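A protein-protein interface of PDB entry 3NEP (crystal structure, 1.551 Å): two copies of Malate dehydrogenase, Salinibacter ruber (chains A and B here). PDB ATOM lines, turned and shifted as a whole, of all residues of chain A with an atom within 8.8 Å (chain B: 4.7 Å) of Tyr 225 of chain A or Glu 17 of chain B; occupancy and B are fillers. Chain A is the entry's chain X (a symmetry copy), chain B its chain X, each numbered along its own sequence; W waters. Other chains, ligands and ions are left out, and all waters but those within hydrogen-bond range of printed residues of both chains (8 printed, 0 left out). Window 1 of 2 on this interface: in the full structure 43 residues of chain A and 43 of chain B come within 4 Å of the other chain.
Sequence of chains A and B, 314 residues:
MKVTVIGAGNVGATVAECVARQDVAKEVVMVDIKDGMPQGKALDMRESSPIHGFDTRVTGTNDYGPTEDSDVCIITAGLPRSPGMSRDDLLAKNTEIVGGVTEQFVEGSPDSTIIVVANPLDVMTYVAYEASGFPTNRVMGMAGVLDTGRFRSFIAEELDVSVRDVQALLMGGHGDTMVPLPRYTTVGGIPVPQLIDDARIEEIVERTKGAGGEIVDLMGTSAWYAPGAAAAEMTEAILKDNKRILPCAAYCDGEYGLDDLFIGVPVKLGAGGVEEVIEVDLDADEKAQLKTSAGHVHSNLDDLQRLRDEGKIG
Printed residues of chain B that touch a printed residue of chain A: Ala 13, Glu 17, Cys 18, Arg 21, Lys 41, Asp 44, Met 45, Ser 48 and His 52.
Hydrophobic or aromatic side chains of chain B that line the printed part of chain A: Ala 13, Met 45 and His 52.
Of the 26 printed residues of chain A, 11 touch a printed residue of chain B.
Hydrophobic or aromatic side chains of chain A within 4 Å of the printed part of chain B: His 52, Ile 215, Met 219, Ala 223, Trp 224, Tyr 225, Ala 226, Pro 227 and Ala 229.
N of Lys 41 of chain B is in hydrogen-bond range of SD of Met 219 of chain A, 3.8 Å away.
The backbone NH of Trp 224 of chain A sits at hydrogen-bond distance from the side-chain carboxylate of Asp 44 of chain B, at 2.8 Å.
The side-chain carboxylate (OD2) of Asp 44 of chain B is in hydrogen-bond range of the backbone NH (N) of Tyr 225 of chain A (2.9 Å).
The backbone NH (N) of Ala 226 of chain A lies within hydrogen-bond range of the side-chain carboxylate (OD1) of Asp 44 of chain B (2.9 Å).
Leu 146 of chain A touches none of the printed residues of chain B.
Of the printed residues of chain B, Met 219 of chain A touches Lys 41.
Printed residues of chain B within 4 Å of Tyr 225 of chain A: Ala 13, Glu 17, Asp 44 and Met 45.
Of the printed residues of chain A, Ala 13 of chain B touches Tyr 225.
No residue of chain A comes within 4 Å of Ala 16 of chain B.
Glu 17 of chain B touches one residue of chain A.
Cys 18 of chain B touches one residue of chain A.
The nearest printed residue of chain B that does not touch Tyr 225 of chain A is Ser 48 of chain B (4.01 Å).
The nearest residue of chain A that does not touch Glu 17 of chain B is Arg 21 of chain A (4.8 Å).
Water W4 bridges the backbone carbonyl oxygen of Cys 18 of chain B and the guanidinium group of Arg 21 of chain A.
Water W1 lies within hydrogen-bond range of a ring nitrogen (NE2) of His 52 of chain B (2.8 Å) and the backbone carbonyl oxygen (O) of Tyr 225 of chain A (2.8 Å).
Water W8 bridges NZ of Lys 41 of chain B (2.9 Å) and OH of Tyr 225 of chain A (2.9 Å).
Arg 21 of chain B touches its own counterpart, Arg 21 of chain A.
Positions printed for both chains: 13, 14, 15, 17, 18, 21 and 52.
Of the 16 pairs that touch across the chains among the printed residues, 3 have their exchanged pair printed and touching as well.
SG of Cys 18 of chain A sits at hydrogen-bond distance from O of Thr 14 of chain A, at 3.3 Å.
NH1 of Arg 21 of chain A lies within salt-bridge range of OE2 of Glu 17 of chain A (2.9 Å).
A ring nitrogen (ND1) of His 52 of chain A sits at hydrogen-bond distance from the guanidinium group (NE) of Arg 21 of chain A (3.5 Å).
Cys 18 of chain B touches His 52 of chain A.
Asp 44 of chain B touches Ala 223 of chain A (OD1 to CB, 3.4 Å).
Lys 41 of chain B touches Trp 224 of chain A (CE to CH2, 3.995 Å).
Tyr 225 of chain A touches Ala 13 of chain B (OH to CB, 3.5 Å).
CB of Ala 229 of chain A touches NE2 of His 52 of chain B, at 3.3 Å.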
ATOM      1  N   ASN A  10      16.864  29.237 -21.730  1.00  0.00           N
ATOM      2  CA  ASN A  10      17.326  27.941 -22.224  1.00  0.00           C
ATOM      3  C   ASN A  10      18.498  28.050 -23.187  1.00  0.00           C
ATOM      4  O   ASN A  10      19.465  27.311 -23.063  1.00  0.00           O
ATOM      5  CB  ASN A  10      16.184  27.188 -22.903  1.00  0.00           C
ATOM      6  CG  ASN A  10      15.070  26.887 -21.959  1.00  0.00           C
ATOM      7  OD1 ASN A  10      15.324  26.567 -20.796  1.00  0.00           O
ATOM      8  ND2 ASN A  10      13.808  26.960 -22.454  1.00  0.00           N
ATOM      9  N   VAL A  11      18.433  28.946 -24.160  1.00  0.00           N
ATOM     10  CA  VAL A  11      19.534  29.005 -25.108  1.00  0.00           C
ATOM     11  C   VAL A  11      20.811  29.552 -24.485  1.00  0.00           C
ATOM     12  O   VAL A  11      21.879  28.963 -24.637  1.00  0.00           O
ATOM     13  CB  VAL A  11      19.148  29.801 -26.365  1.00  0.00           C
ATOM     14  CG1 VAL A  11      20.282  29.843 -27.315  1.00  0.00           C
ATOM     15  CG2 VAL A  11      17.950  29.165 -27.017  1.00  0.00           C
ATOM     16  N   GLY A  12      20.698  30.654 -23.756  1.00  0.00           N
ATOM     17  CA  GLY A  12      21.868  31.304 -23.182  1.00  0.00           C
ATOM     18  C   GLY A  12      22.567  30.392 -22.177  1.00  0.00           C
ATOM     19  O   GLY A  12      23.770  30.268 -22.156  1.00  0.00           O
ATOM     20  N   ALA A  13      21.784  29.774 -21.328  1.00  0.00           N
ATOM     21  CA  ALA A  13      22.331  28.853 -20.328  1.00  0.00           C
ATOM     22  C   ALA A  13      23.036  27.671 -21.005  1.00  0.00           C
ATOM     23  O   ALA A  13      24.051  27.191 -20.538  1.00  0.00           O
ATOM     24  CB  ALA A  13      21.213  28.366 -19.389  1.00  0.00           C
ATOM     25  N   THR A  14      22.489  27.200 -22.113  1.00  0.00           N
ATOM     26  CA  THR A  14      23.128  26.140 -22.880  1.00  0.00           C
ATOM     27  C   THR A  14      24.452  26.599 -23.471  1.00  0.00           C
ATOM     28  O   THR A  14      25.459  25.859 -23.406  1.00  0.00           O
ATOM     29  CB  THR A  14      22.209  25.615 -23.999  1.00  0.00           C
ATOM     30  OG1 THR A  14      21.034  25.067 -23.405  1.00  0.00           O
ATOM     31  CG2 THR A  14      22.888  24.489 -24.780  1.00  0.00           C
ATOM     32  N   VAL A  15      24.475  27.820 -24.016  1.00  0.00           N
ATOM     33  CA  VAL A  15      25.755  28.350 -24.494  1.00  0.00           C
ATOM     34  C   VAL A  15      26.760  28.369 -23.351  1.00  0.00           C
ATOM     35  O   VAL A  15      27.880  27.931 -23.502  1.00  0.00           O
ATOM     36  CB  VAL A  15      25.624  29.748 -25.052  1.00  0.00           C
ATOM     37  CG1 VAL A  15      26.989  30.295 -25.421  1.00  0.00           C
ATOM     38  CG2 VAL A  15      24.719  29.731 -26.254  1.00  0.00           C
ATOM     39  N   GLU A  17      26.934  26.771 -20.415  1.00  0.00           N
ATOM     40  CA  GLU A  17      27.333  25.466 -19.923  1.00  0.00           C
ATOM     41  C   GLU A  17      28.222  24.754 -20.944  1.00  0.00           C
ATOM     42  O   GLU A  17      29.195  24.081 -20.568  1.00  0.00           O
ATOM     43  CB  GLU A  17      26.101  24.626 -19.609  1.00  0.00           C
ATOM     44  CG  GLU A  17      26.381  23.478 -18.631  1.00  0.00           C
ATOM     45  CD  GLU A  17      26.634  22.151 -19.260  1.00  0.00           C
ATOM     46  OE1 GLU A  17      26.129  21.884 -20.390  1.00  0.00           O
ATOM     47  OE2 GLU A  17      27.300  21.332 -18.560  1.00  0.00           O
ATOM     48  N   CYS A  18      27.900  24.874 -22.227  1.00  0.00           N
ATOM     49  CA  CYS A  18      28.730  24.229 -23.252  1.00  0.00           C
ATOM     50  C   CYS A  18      30.141  24.868 -23.265  1.00  0.00           C
ATOM     51  O   CYS A  18      31.143  24.167 -23.339  1.00  0.00           O
ATOM     52  CB  CYS A  18      28.132  24.402 -24.660  1.00  0.00           C
ATOM     53  SG  CYS A  18      26.729  23.306 -25.013  1.00  0.00           S
ATOM     54  N   ARG A  21      32.052  23.675 -20.149  1.00  0.00           N
ATOM     55  CA  ARG A  21      32.492  22.272 -20.283  1.00  0.00           C
ATOM     56  C   ARG A  21      33.754  22.116 -21.125  1.00  0.00           C
ATOM     57  O   ARG A  21      34.514  21.175 -20.900  1.00  0.00           O
ATOM     58  CB  ARG A  21      31.349  21.424 -20.907  1.00  0.00           C
ATOM     59  CG  ARG A  21      30.152  21.304 -19.996  1.00  0.00           C
ATOM     60  CD  ARG A  21      30.169  20.057 -19.219  1.00  0.00           C
ATOM     61  NE  ARG A  21      30.009  18.850 -20.033  1.00  0.00           N
ATOM     62  CZ  ARG A  21      28.844  18.317 -20.409  1.00  0.00           C
ATOM     63  NH1 ARG A  21      27.688  18.901 -20.143  1.00  0.00           N
ATOM     64  NH2 ARG A  21      28.853  17.203 -21.088  1.00  0.00           N
ATOM     65  N   HIS A  52      31.690  16.872 -13.963  1.00  0.00           N
ATOM     66  CA  HIS A  52      32.166  16.896 -15.338  1.00  0.00           C
ATOM     67  C   HIS A  52      33.684  17.073 -15.460  1.00  0.00           C
ATOM     68  O   HIS A  52      34.287  16.569 -16.411  1.00  0.00           O
ATOM     69  CB  HIS A  52      31.479  18.047 -16.084  1.00  0.00           C
ATOM     70  CG  HIS A  52      30.051  17.777 -16.437  1.00  0.00           C
ATOM     71  ND1 HIS A  52      29.672  16.755 -17.273  1.00  0.00           N
ATOM     72  CD2 HIS A  52      28.928  18.463 -16.136  1.00  0.00           C
ATOM     73  CE1 HIS A  52      28.356  16.782 -17.425  1.00  0.00           C
ATOM     74  NE2 HIS A  52      27.884  17.814 -16.753  1.00  0.00           N
ATOM     75  N   MET A 142      24.849  33.793 -35.219  1.00  0.00           N
ATOM     76  CA  MET A 142      24.798  32.344 -35.319  1.00  0.00           C
ATOM     77  C   MET A 142      23.503  31.981 -36.066  1.00  0.00           C
ATOM     78  O   MET A 142      22.410  32.308 -35.612  1.00  0.00           O
ATOM     79  CB  MET A 142      24.764  31.690 -33.922  1.00  0.00           C
ATOM     80  CG  MET A 142      24.944  30.156 -33.953  1.00  0.00           C
ATOM     81  SD  MET A 142      23.470  29.285 -34.582  1.00  0.00           S
ATOM     82  CE  MET A 142      22.331  29.484 -33.229  1.00  0.00           C
ATOM     83  N   LEU A 146      23.825  26.079 -36.883  1.00  0.00           N
ATOM     84  CA  LEU A 146      22.621  25.360 -36.483  1.00  0.00           C
ATOM     85  C   LEU A 146      21.910  24.697 -37.679  1.00  0.00           C
ATOM     86  O   LEU A 146      21.521  23.532 -37.601  1.00  0.00           O
ATOM     87  CB  LEU A 146      21.684  26.309 -35.787  1.00  0.00           C
ATOM     88  CG  LEU A 146      20.278  25.791 -35.451  1.00  0.00           C
ATOM     89  CD1 LEU A 146      20.361  24.622 -34.435  1.00  0.00           C
ATOM     90  CD2 LEU A 146      19.458  26.921 -34.852  1.00  0.00           C
ATOM     91  N   ARG A 150      21.609  20.638 -38.317  1.00  0.00           N
ATOM     92  CA  ARG A 150      20.317  19.992 -38.599  1.00  0.00           C
ATOM     93  C   ARG A 150      20.359  19.174 -39.889  1.00  0.00           C
ATOM     94  O   ARG A 150      20.069  17.985 -39.880  1.00  0.00           O
ATOM     95  CB  ARG A 150      19.215  21.045 -38.660  1.00  0.00           C
ATOM     96  CG  ARG A 150      18.901  21.644 -37.297  1.00  0.00           C
ATOM     97  CD  ARG A 150      17.958  22.866 -37.378  1.00  0.00           C
ATOM     98  NE  ARG A 150      17.407  23.103 -36.050  1.00  0.00           N
ATOM     99  CZ  ARG A 150      16.845  24.245 -35.654  1.00  0.00           C
ATOM    100  NH1 ARG A 150      16.702  25.267 -36.502  1.00  0.00           N
ATOM    101  NH2 ARG A 150      16.374  24.358 -34.411  1.00  0.00           N
ATOM    102  N   ILE A 215      10.058  21.736 -34.078  1.00  0.00           N
ATOM    103  CA  ILE A 215      10.267  21.521 -32.650  1.00  0.00           C
ATOM    104  C   ILE A 215       9.236  22.298 -31.831  1.00  0.00           C
ATOM    105  O   ILE A 215       8.655  21.773 -30.882  1.00  0.00           O
ATOM    106  CB  ILE A 215      11.713  21.887 -32.271  1.00  0.00           C
ATOM    107  CG1 ILE A 215      12.661  20.785 -32.799  1.00  0.00           C
ATOM    108  CG2 ILE A 215      11.837  22.003 -30.757  1.00  0.00           C
ATOM    109  CD1 ILE A 215      14.074  21.107 -32.674  1.00  0.00           C
ATOM    110  N   MET A 219       6.789  20.485 -29.000  1.00  0.00           N
ATOM    111  CA  MET A 219       6.873  20.697 -27.542  1.00  0.00           C
ATOM    112  C   MET A 219       6.382  22.054 -27.051  1.00  0.00           C
ATOM    113  O   MET A 219       6.335  22.327 -25.838  1.00  0.00           O
ATOM    114  CB  MET A 219       8.287  20.409 -27.029  1.00  0.00           C
ATOM    115  CG  MET A 219       9.383  21.330 -27.519  1.00  0.00           C
ATOM    116  SD  MET A 219      10.965  20.756 -26.874  1.00  0.00           S
ATOM    117  CE  MET A 219      12.004  22.205 -27.180  1.00  0.00           C
ATOM    118  N   SER A 222      10.664  26.836 -28.362  1.00  0.00           N
ATOM    119  CA  SER A 222      11.755  26.649 -29.334  1.00  0.00           C
ATOM    120  C   SER A 222      12.972  25.899 -28.761  1.00  0.00           C
ATOM    121  O   SER A 222      13.152  25.768 -27.543  1.00  0.00           O
ATOM    122  CB  SER A 222      12.172  27.994 -29.931  1.00  0.00           C
ATOM    123  OG  SER A 222      12.347  28.920 -28.912  1.00  0.00           O
ATOM    124  N   ALA A 223      13.797  25.413 -29.675  1.00  0.00           N
ATOM    125  CA  ALA A 223      14.939  24.589 -29.364  1.00  0.00           C
ATOM    126  C   ALA A 223      16.010  25.326 -28.592  1.00  0.00           C
ATOM    127  O   ALA A 223      16.084  26.583 -28.632  1.00  0.00           O
ATOM    128  CB  ALA A 223      15.552  24.042 -30.664  1.00  0.00           C
ATOM    129  N   TRP A 224      16.853  24.544 -27.900  1.00  0.00           N
ATOM    130  CA  TRP A 224      18.030  25.125 -27.304  1.00  0.00           C
ATOM    131  C   TRP A 224      19.309  24.293 -27.318  1.00  0.00           C
ATOM    132  O   TRP A 224      20.402  24.870 -27.264  1.00  0.00           O
ATOM    133  CB  TRP A 224      17.731  25.547 -25.851  1.00  0.00           C
ATOM    134  CG  TRP A 224      17.305  24.439 -24.905  1.00  0.00           C
ATOM    135  CD1 TRP A 224      18.109  23.693 -24.094  1.00  0.00           C
ATOM    136  CD2 TRP A 224      15.972  24.050 -24.594  1.00  0.00           C
ATOM    137  NE1 TRP A 224      17.361  22.842 -23.325  1.00  0.00           N
ATOM    138  CE2 TRP A 224      16.039  23.056 -23.607  1.00  0.00           C
ATOM    139  CE3 TRP A 224      14.717  24.451 -25.060  1.00  0.00           C
ATOM    140  CZ2 TRP A 224      14.913  22.445 -23.094  1.00  0.00           C
ATOM    141  CZ3 TRP A 224      13.622  23.852 -24.557  1.00  0.00           C
ATOM    142  CH2 TRP A 224      13.710  22.857 -23.573  1.00  0.00           C
ATOM    143  N   TYR A 225      19.206  22.967 -27.352  1.00  0.00           N
ATOM    144  CA  TYR A 225      20.422  22.145 -27.313  1.00  0.00           C
ATOM    145  C   TYR A 225      21.263  22.399 -28.536  1.00  0.00           C
ATOM    146  O   TYR A 225      22.481  22.645 -28.437  1.00  0.00           O
ATOM    147  CB  TYR A 225      20.077  20.642 -27.192  1.00  0.00           C
ATOM    148  CG  TYR A 225      19.560  20.270 -25.824  1.00  0.00           C
ATOM    149  CD1 TYR A 225      18.226  19.966 -25.603  1.00  0.00           C
ATOM    150  CD2 TYR A 225      20.422  20.271 -24.739  1.00  0.00           C
ATOM    151  CE1 TYR A 225      17.769  19.620 -24.319  1.00  0.00           C
ATOM    152  CE2 TYR A 225      19.969  19.936 -23.467  1.00  0.00           C
ATOM    153  CZ  TYR A 225      18.648  19.617 -23.273  1.00  0.00           C
ATOM    154  OH  TYR A 225      18.185  19.304 -22.012  1.00  0.00           O
ATOM    155  N   ALA A 226      20.633  22.325 -29.704  1.00  0.00           N
ATOM    156  CA  ALA A 226      21.410  22.529 -30.900  1.00  0.00           C
ATOM    157  C   ALA A 226      21.796  24.011 -31.132  1.00  0.00           C
ATOM    158  O   ALA A 226      22.936  24.290 -31.489  1.00  0.00           O
ATOM    159  CB  ALA A 226      20.688  21.917 -32.156  1.00  0.00           C
ATOM    160  N   PRO A 227      20.870  24.974 -30.933  1.00  0.00           N
ATOM    161  CA  PRO A 227      21.267  26.383 -31.056  1.00  0.00           C
ATOM    162  C   PRO A 227      22.396  26.748 -30.095  1.00  0.00           C
ATOM    163  O   PRO A 227      23.356  27.417 -30.472  1.00  0.00           O
ATOM    164  CB  PRO A 227      19.989  27.154 -30.721  1.00  0.00           C
ATOM    165  CG  PRO A 227      18.867  26.226 -31.098  1.00  0.00           C
ATOM    166  CD  PRO A 227      19.421  24.809 -30.804  1.00  0.00           C
ATOM    167  N   GLY A 228      22.312  26.262 -28.864  1.00  0.00           N
ATOM    168  CA  GLY A 228      23.368  26.553 -27.905  1.00  0.00           C
ATOM    169  C   GLY A 228      24.697  25.946 -28.277  1.00  0.00           C
ATOM    170  O   GLY A 228      25.725  26.596 -28.128  1.00  0.00           O
ATOM    171  N   ALA A 229      24.676  24.686 -28.738  1.00  0.00           N
ATOM    172  CA  ALA A 229      25.891  24.034 -29.171  1.00  0.00           C
ATOM    173  C   ALA A 229      26.524  24.815 -30.314  1.00  0.00           C
ATOM    174  O   ALA A 229      27.749  24.949 -30.351  1.00  0.00           O
ATOM    175  CB  ALA A 229      25.631  22.602 -29.591  1.00  0.00           C
ATOM    176  N   ALA A 230      25.704  25.315 -31.254  1.00  0.00           N
ATOM    177  CA  ALA A 230      26.218  25.991 -32.406  1.00  0.00           C
ATOM    178  C   ALA A 230      26.950  27.289 -32.016  1.00  0.00           C
ATOM    179  O   ALA A 230      28.066  27.577 -32.516  1.00  0.00           O
ATOM    180  CB  ALA A 230      25.052  26.280 -33.350  1.00  0.00           C
ATOM    181  N   ALA A 231      26.353  28.064 -31.128  1.00  0.00           N
ATOM    182  CA  ALA A 231      26.998  29.308 -30.686  1.00  0.00           C
ATOM    183  C   ALA A 231      28.243  29.035 -29.851  1.00  0.00           C
ATOM    184  O   ALA A 231      29.242  29.772 -29.942  1.00  0.00           O
ATOM    185  CB  ALA A 231      26.015  30.203 -29.923  1.00  0.00           C
ATOM    186  N   ALA A 232      28.227  27.945 -29.088  1.00  0.00           N
ATOM    187  CA  ALA A 232      29.404  27.580 -28.344  1.00  0.00           C
ATOM    188  C   ALA A 232      30.545  27.150 -29.245  1.00  0.00           C
ATOM    189  O   ALA A 232      31.709  27.416 -28.931  1.00  0.00           O
ATOM    190  CB  ALA A 232      29.051  26.468 -27.302  1.00  0.00           C
ATOM    191  N   ALA B  13      16.132  15.080 -19.048  1.00  0.00           N
ATOM    192  CA  ALA B  13      16.716  15.524 -20.317  1.00  0.00           C
ATOM    193  C   ALA B  13      18.221  15.775 -20.164  1.00  0.00           C
ATOM    194  O   ALA B  13      19.000  15.498 -21.057  1.00  0.00           O
ATOM    195  CB  ALA B  13      15.993  16.787 -20.819  1.00  0.00           C
ATOM    196  N   THR B  14      18.630  16.304 -19.024  1.00  0.00           N
ATOM    197  CA  THR B  14      20.046  16.498 -18.744  1.00  0.00           C
ATOM    198  C   THR B  14      20.782  15.171 -18.642  1.00  0.00           C
ATOM    199  O   THR B  14      21.887  15.021 -19.208  1.00  0.00           O
ATOM    200  CB  THR B  14      20.265  17.319 -17.459  1.00  0.00           C
ATOM    201  OG1 THR B  14      19.681  18.607 -17.635  1.00  0.00           O
ATOM    202  CG2 THR B  14      21.755  17.529 -17.193  1.00  0.00           C
ATOM    203  N   VAL B  15      20.172  14.197 -17.958  1.00  0.00           N
ATOM    204  CA  VAL B  15      20.788  12.868 -17.930  1.00  0.00           C
ATOM    205  C   VAL B  15      20.959  12.354 -19.352  1.00  0.00           C
ATOM    206  O   VAL B  15      22.011  11.876 -19.717  1.00  0.00           O
ATOM    207  CB  VAL B  15      19.966  11.872 -17.145  1.00  0.00           C
ATOM    208  CG1 VAL B  15      20.582  10.490 -17.247  1.00  0.00           C
ATOM    209  CG2 VAL B  15      19.879  12.307 -15.708  1.00  0.00           C
ATOM    210  N   ALA B  16      19.896  12.415 -20.135  1.00  0.00           N
ATOM    211  CA  ALA B  16      19.919  11.879 -21.487  1.00  0.00           C
ATOM    212  C   ALA B  16      21.004  12.536 -22.338  1.00  0.00           C
ATOM    213  O   ALA B  16      21.744  11.856 -23.030  1.00  0.00           O
ATOM    214  CB  ALA B  16      18.557  12.080 -22.160  1.00  0.00           C
ATOM    215  N   GLU B  17      21.029  13.849 -22.346  1.00  0.00           N
ATOM    216  CA  GLU B  17      21.979  14.585 -23.158  1.00  0.00           C
ATOM    217  C   GLU B  17      23.410  14.319 -22.688  1.00  0.00           C
ATOM    218  O   GLU B  17      24.329  14.194 -23.513  1.00  0.00           O
ATOM    219  CB  GLU B  17      21.668  16.076 -23.106  1.00  0.00           C
ATOM    220  CG  GLU B  17      22.249  16.860 -24.288  1.00  0.00           C
ATOM    221  CD  GLU B  17      23.555  17.531 -24.029  1.00  0.00           C
ATOM    222  OE1 GLU B  17      23.858  17.883 -22.852  1.00  0.00           O
ATOM    223  OE2 GLU B  17      24.258  17.772 -25.054  1.00  0.00           O
ATOM    224  N   CYS B  18      23.621  14.246 -21.379  1.00  0.00           N
ATOM    225  CA  CYS B  18      24.971  13.972 -20.871  1.00  0.00           C
ATOM    226  C   CYS B  18      25.417  12.551 -21.298  1.00  0.00           C
ATOM    227  O   CYS B  18      26.546  12.353 -21.731  1.00  0.00           O
ATOM    228  CB  CYS B  18      25.024  14.029 -19.333  1.00  0.00           C
ATOM    229  SG  CYS B  18      25.038  15.710 -18.651  1.00  0.00           S
ATOM    230  N   VAL B  19      24.534  11.556 -21.192  1.00  0.00           N
ATOM    231  CA  VAL B  19      24.902  10.197 -21.617  1.00  0.00           C
ATOM    232  C   VAL B  19      25.166  10.171 -23.129  1.00  0.00           C
ATOM    233  O   VAL B  19      26.141   9.534 -23.588  1.00  0.00           O
ATOM    234  CB  VAL B  19      23.809   9.174 -21.224  1.00  0.00           C
ATOM    235  CG1 VAL B  19      24.117   7.814 -21.825  1.00  0.00           C
ATOM    236  CG2 VAL B  19      23.708   9.085 -19.697  1.00  0.00           C
ATOM    237  N   ALA B  20      24.342  10.867 -23.898  1.00  0.00           N
ATOM    238  CA  ALA B  20      24.507  10.878 -25.342  1.00  0.00           C
ATOM    239  C   ALA B  20      25.852  11.518 -25.720  1.00  0.00           C
ATOM    240  O   ALA B  20      26.564  11.000 -26.557  1.00  0.00           O
ATOM    241  CB  ALA B  20      23.371  11.630 -26.009  1.00  0.00           C
ATOM    242  N   ARG B  21      26.219  12.600 -25.059  1.00  0.00           N
ATOM    243  CA  ARG B  21      27.502  13.277 -25.334  1.00  0.00           C
ATOM    244  C   ARG B  21      28.716  12.390 -25.080  1.00  0.00           C
ATOM    245  O   ARG B  21      29.743  12.577 -25.729  1.00  0.00           O
ATOM    246  CB  ARG B  21      27.611  14.560 -24.464  1.00  0.00           C
ATOM    247  CG  ARG B  21      26.601  15.611 -24.851  1.00  0.00           C
ATOM    248  CD  ARG B  21      27.164  16.614 -25.766  1.00  0.00           C
ATOM    249  NE  ARG B  21      28.202  17.450 -25.161  1.00  0.00           N
ATOM    250  CZ  ARG B  21      27.988  18.564 -24.457  1.00  0.00           C
ATOM    251  NH1 ARG B  21      26.769  18.982 -24.159  1.00  0.00           N
ATOM    252  NH2 ARG B  21      29.015  19.242 -24.024  1.00  0.00           N
ATOM    253  N   LYS B  41      12.467  17.358 -27.418  1.00  0.00           N
ATOM    254  CA  LYS B  41      13.801  17.430 -26.827  1.00  0.00           C
ATOM    255  C   LYS B  41      14.777  16.462 -27.516  1.00  0.00           C
ATOM    256  O   LYS B  41      15.948  16.814 -27.710  1.00  0.00           O
ATOM    257  CB  LYS B  41      13.730  17.143 -25.328  1.00  0.00           C
ATOM    258  CG  LYS B  41      13.056  18.296 -24.565  1.00  0.00           C
ATOM    259  CD  LYS B  41      13.356  18.163 -23.058  1.00  0.00           C
ATOM    260  CE  LYS B  41      12.621  19.236 -22.283  1.00  0.00           C
ATOM    261  NZ  LYS B  41      12.987  19.196 -20.844  1.00  0.00           N
ATOM    262  N   ASP B  44      15.818  17.888 -30.853  1.00  0.00           N
ATOM    263  CA  ASP B  44      16.757  18.965 -30.653  1.00  0.00           C
ATOM    264  C   ASP B  44      18.145  18.362 -30.341  1.00  0.00           C
ATOM    265  O   ASP B  44      19.172  18.764 -30.898  1.00  0.00           O
ATOM    266  CB  ASP B  44      16.225  19.827 -29.479  1.00  0.00           C
ATOM    267  CG  ASP B  44      17.014  21.109 -29.244  1.00  0.00           C
ATOM    268  OD1 ASP B  44      17.832  21.564 -30.117  1.00  0.00           O
ATOM    269  OD2 ASP B  44      16.766  21.709 -28.176  1.00  0.00           O
ATOM    270  N   MET B  45      18.188  17.361 -29.475  1.00  0.00           N
ATOM    271  CA  MET B  45      19.480  16.704 -29.188  1.00  0.00           C
ATOM    272  C   MET B  45      20.072  16.022 -30.435  1.00  0.00           C
ATOM    273  O   MET B  45      21.277  16.082 -30.673  1.00  0.00           O
ATOM    274  CB  MET B  45      19.350  15.694 -28.032  1.00  0.00           C
ATOM    275  CG  MET B  45      18.908  16.342 -26.749  1.00  0.00           C
ATOM    276  SD  MET B  45      18.779  15.064 -25.461  1.00  0.00           S
ATOM    277  CE  MET B  45      17.883  16.033 -24.274  1.00  0.00           C
ATOM    278  N   SER B  48      21.697  18.465 -32.548  1.00  0.00           N
ATOM    279  CA  SER B  48      22.971  18.919 -31.971  1.00  0.00           C
ATOM    280  C   SER B  48      24.100  17.934 -32.160  1.00  0.00           C
ATOM    281  O   SER B  48      25.285  18.307 -31.965  1.00  0.00           O
ATOM    282  CB  SER B  48      22.814  19.193 -30.457  1.00  0.00           C
ATOM    283  OG  SER B  48      22.932  17.995 -29.683  1.00  0.00           O
ATOM    284  N   HIS B  52      28.261  18.695 -31.643  1.00  0.00           N
ATOM    285  CA  HIS B  52      29.070  18.129 -30.573  1.00  0.00           C
ATOM    286  C   HIS B  52      29.938  16.946 -31.018  1.00  0.00           C
ATOM    287  O   HIS B  52      31.022  16.740 -30.467  1.00  0.00           O
ATOM    288  CB  HIS B  52      28.144  17.658 -29.445  1.00  0.00           C
ATOM    289  CG  HIS B  52      27.577  18.769 -28.618  1.00  0.00           C
ATOM    290  ND1 HIS B  52      28.361  19.620 -27.878  1.00  0.00           N
ATOM    291  CD2 HIS B  52      26.296  19.096 -28.349  1.00  0.00           C
ATOM    292  CE1 HIS B  52      27.585  20.475 -27.230  1.00  0.00           C
ATOM    293  NE2 HIS B  52      26.328  20.171 -27.491  1.00  0.00           N
HETATM  294  O   HOH W   1      23.913  21.166 -26.521  1.00  0.00           O
HETATM  295  O   HOH W   2      17.436  22.024 -32.751  1.00  0.00           O
HETATM  296  O   HOH W   3      19.992  19.748 -20.118  1.00  0.00           O
HETATM  297  O   HOH W   4      28.402  14.146 -20.912  1.00  0.00           O
HETATM  298  O   HOH W   5      25.978  17.293 -21.428  1.00  0.00           O
HETATM  299  O   HOH W   6      30.756  21.755 -24.506  1.00  0.00           O
HETATM  300  O   HOH W   7      27.300  21.086 -22.595  1.00  0.00           O
HETATM  301  O   HOH W   8      15.721  20.047 -20.695  1.00  0.00           O
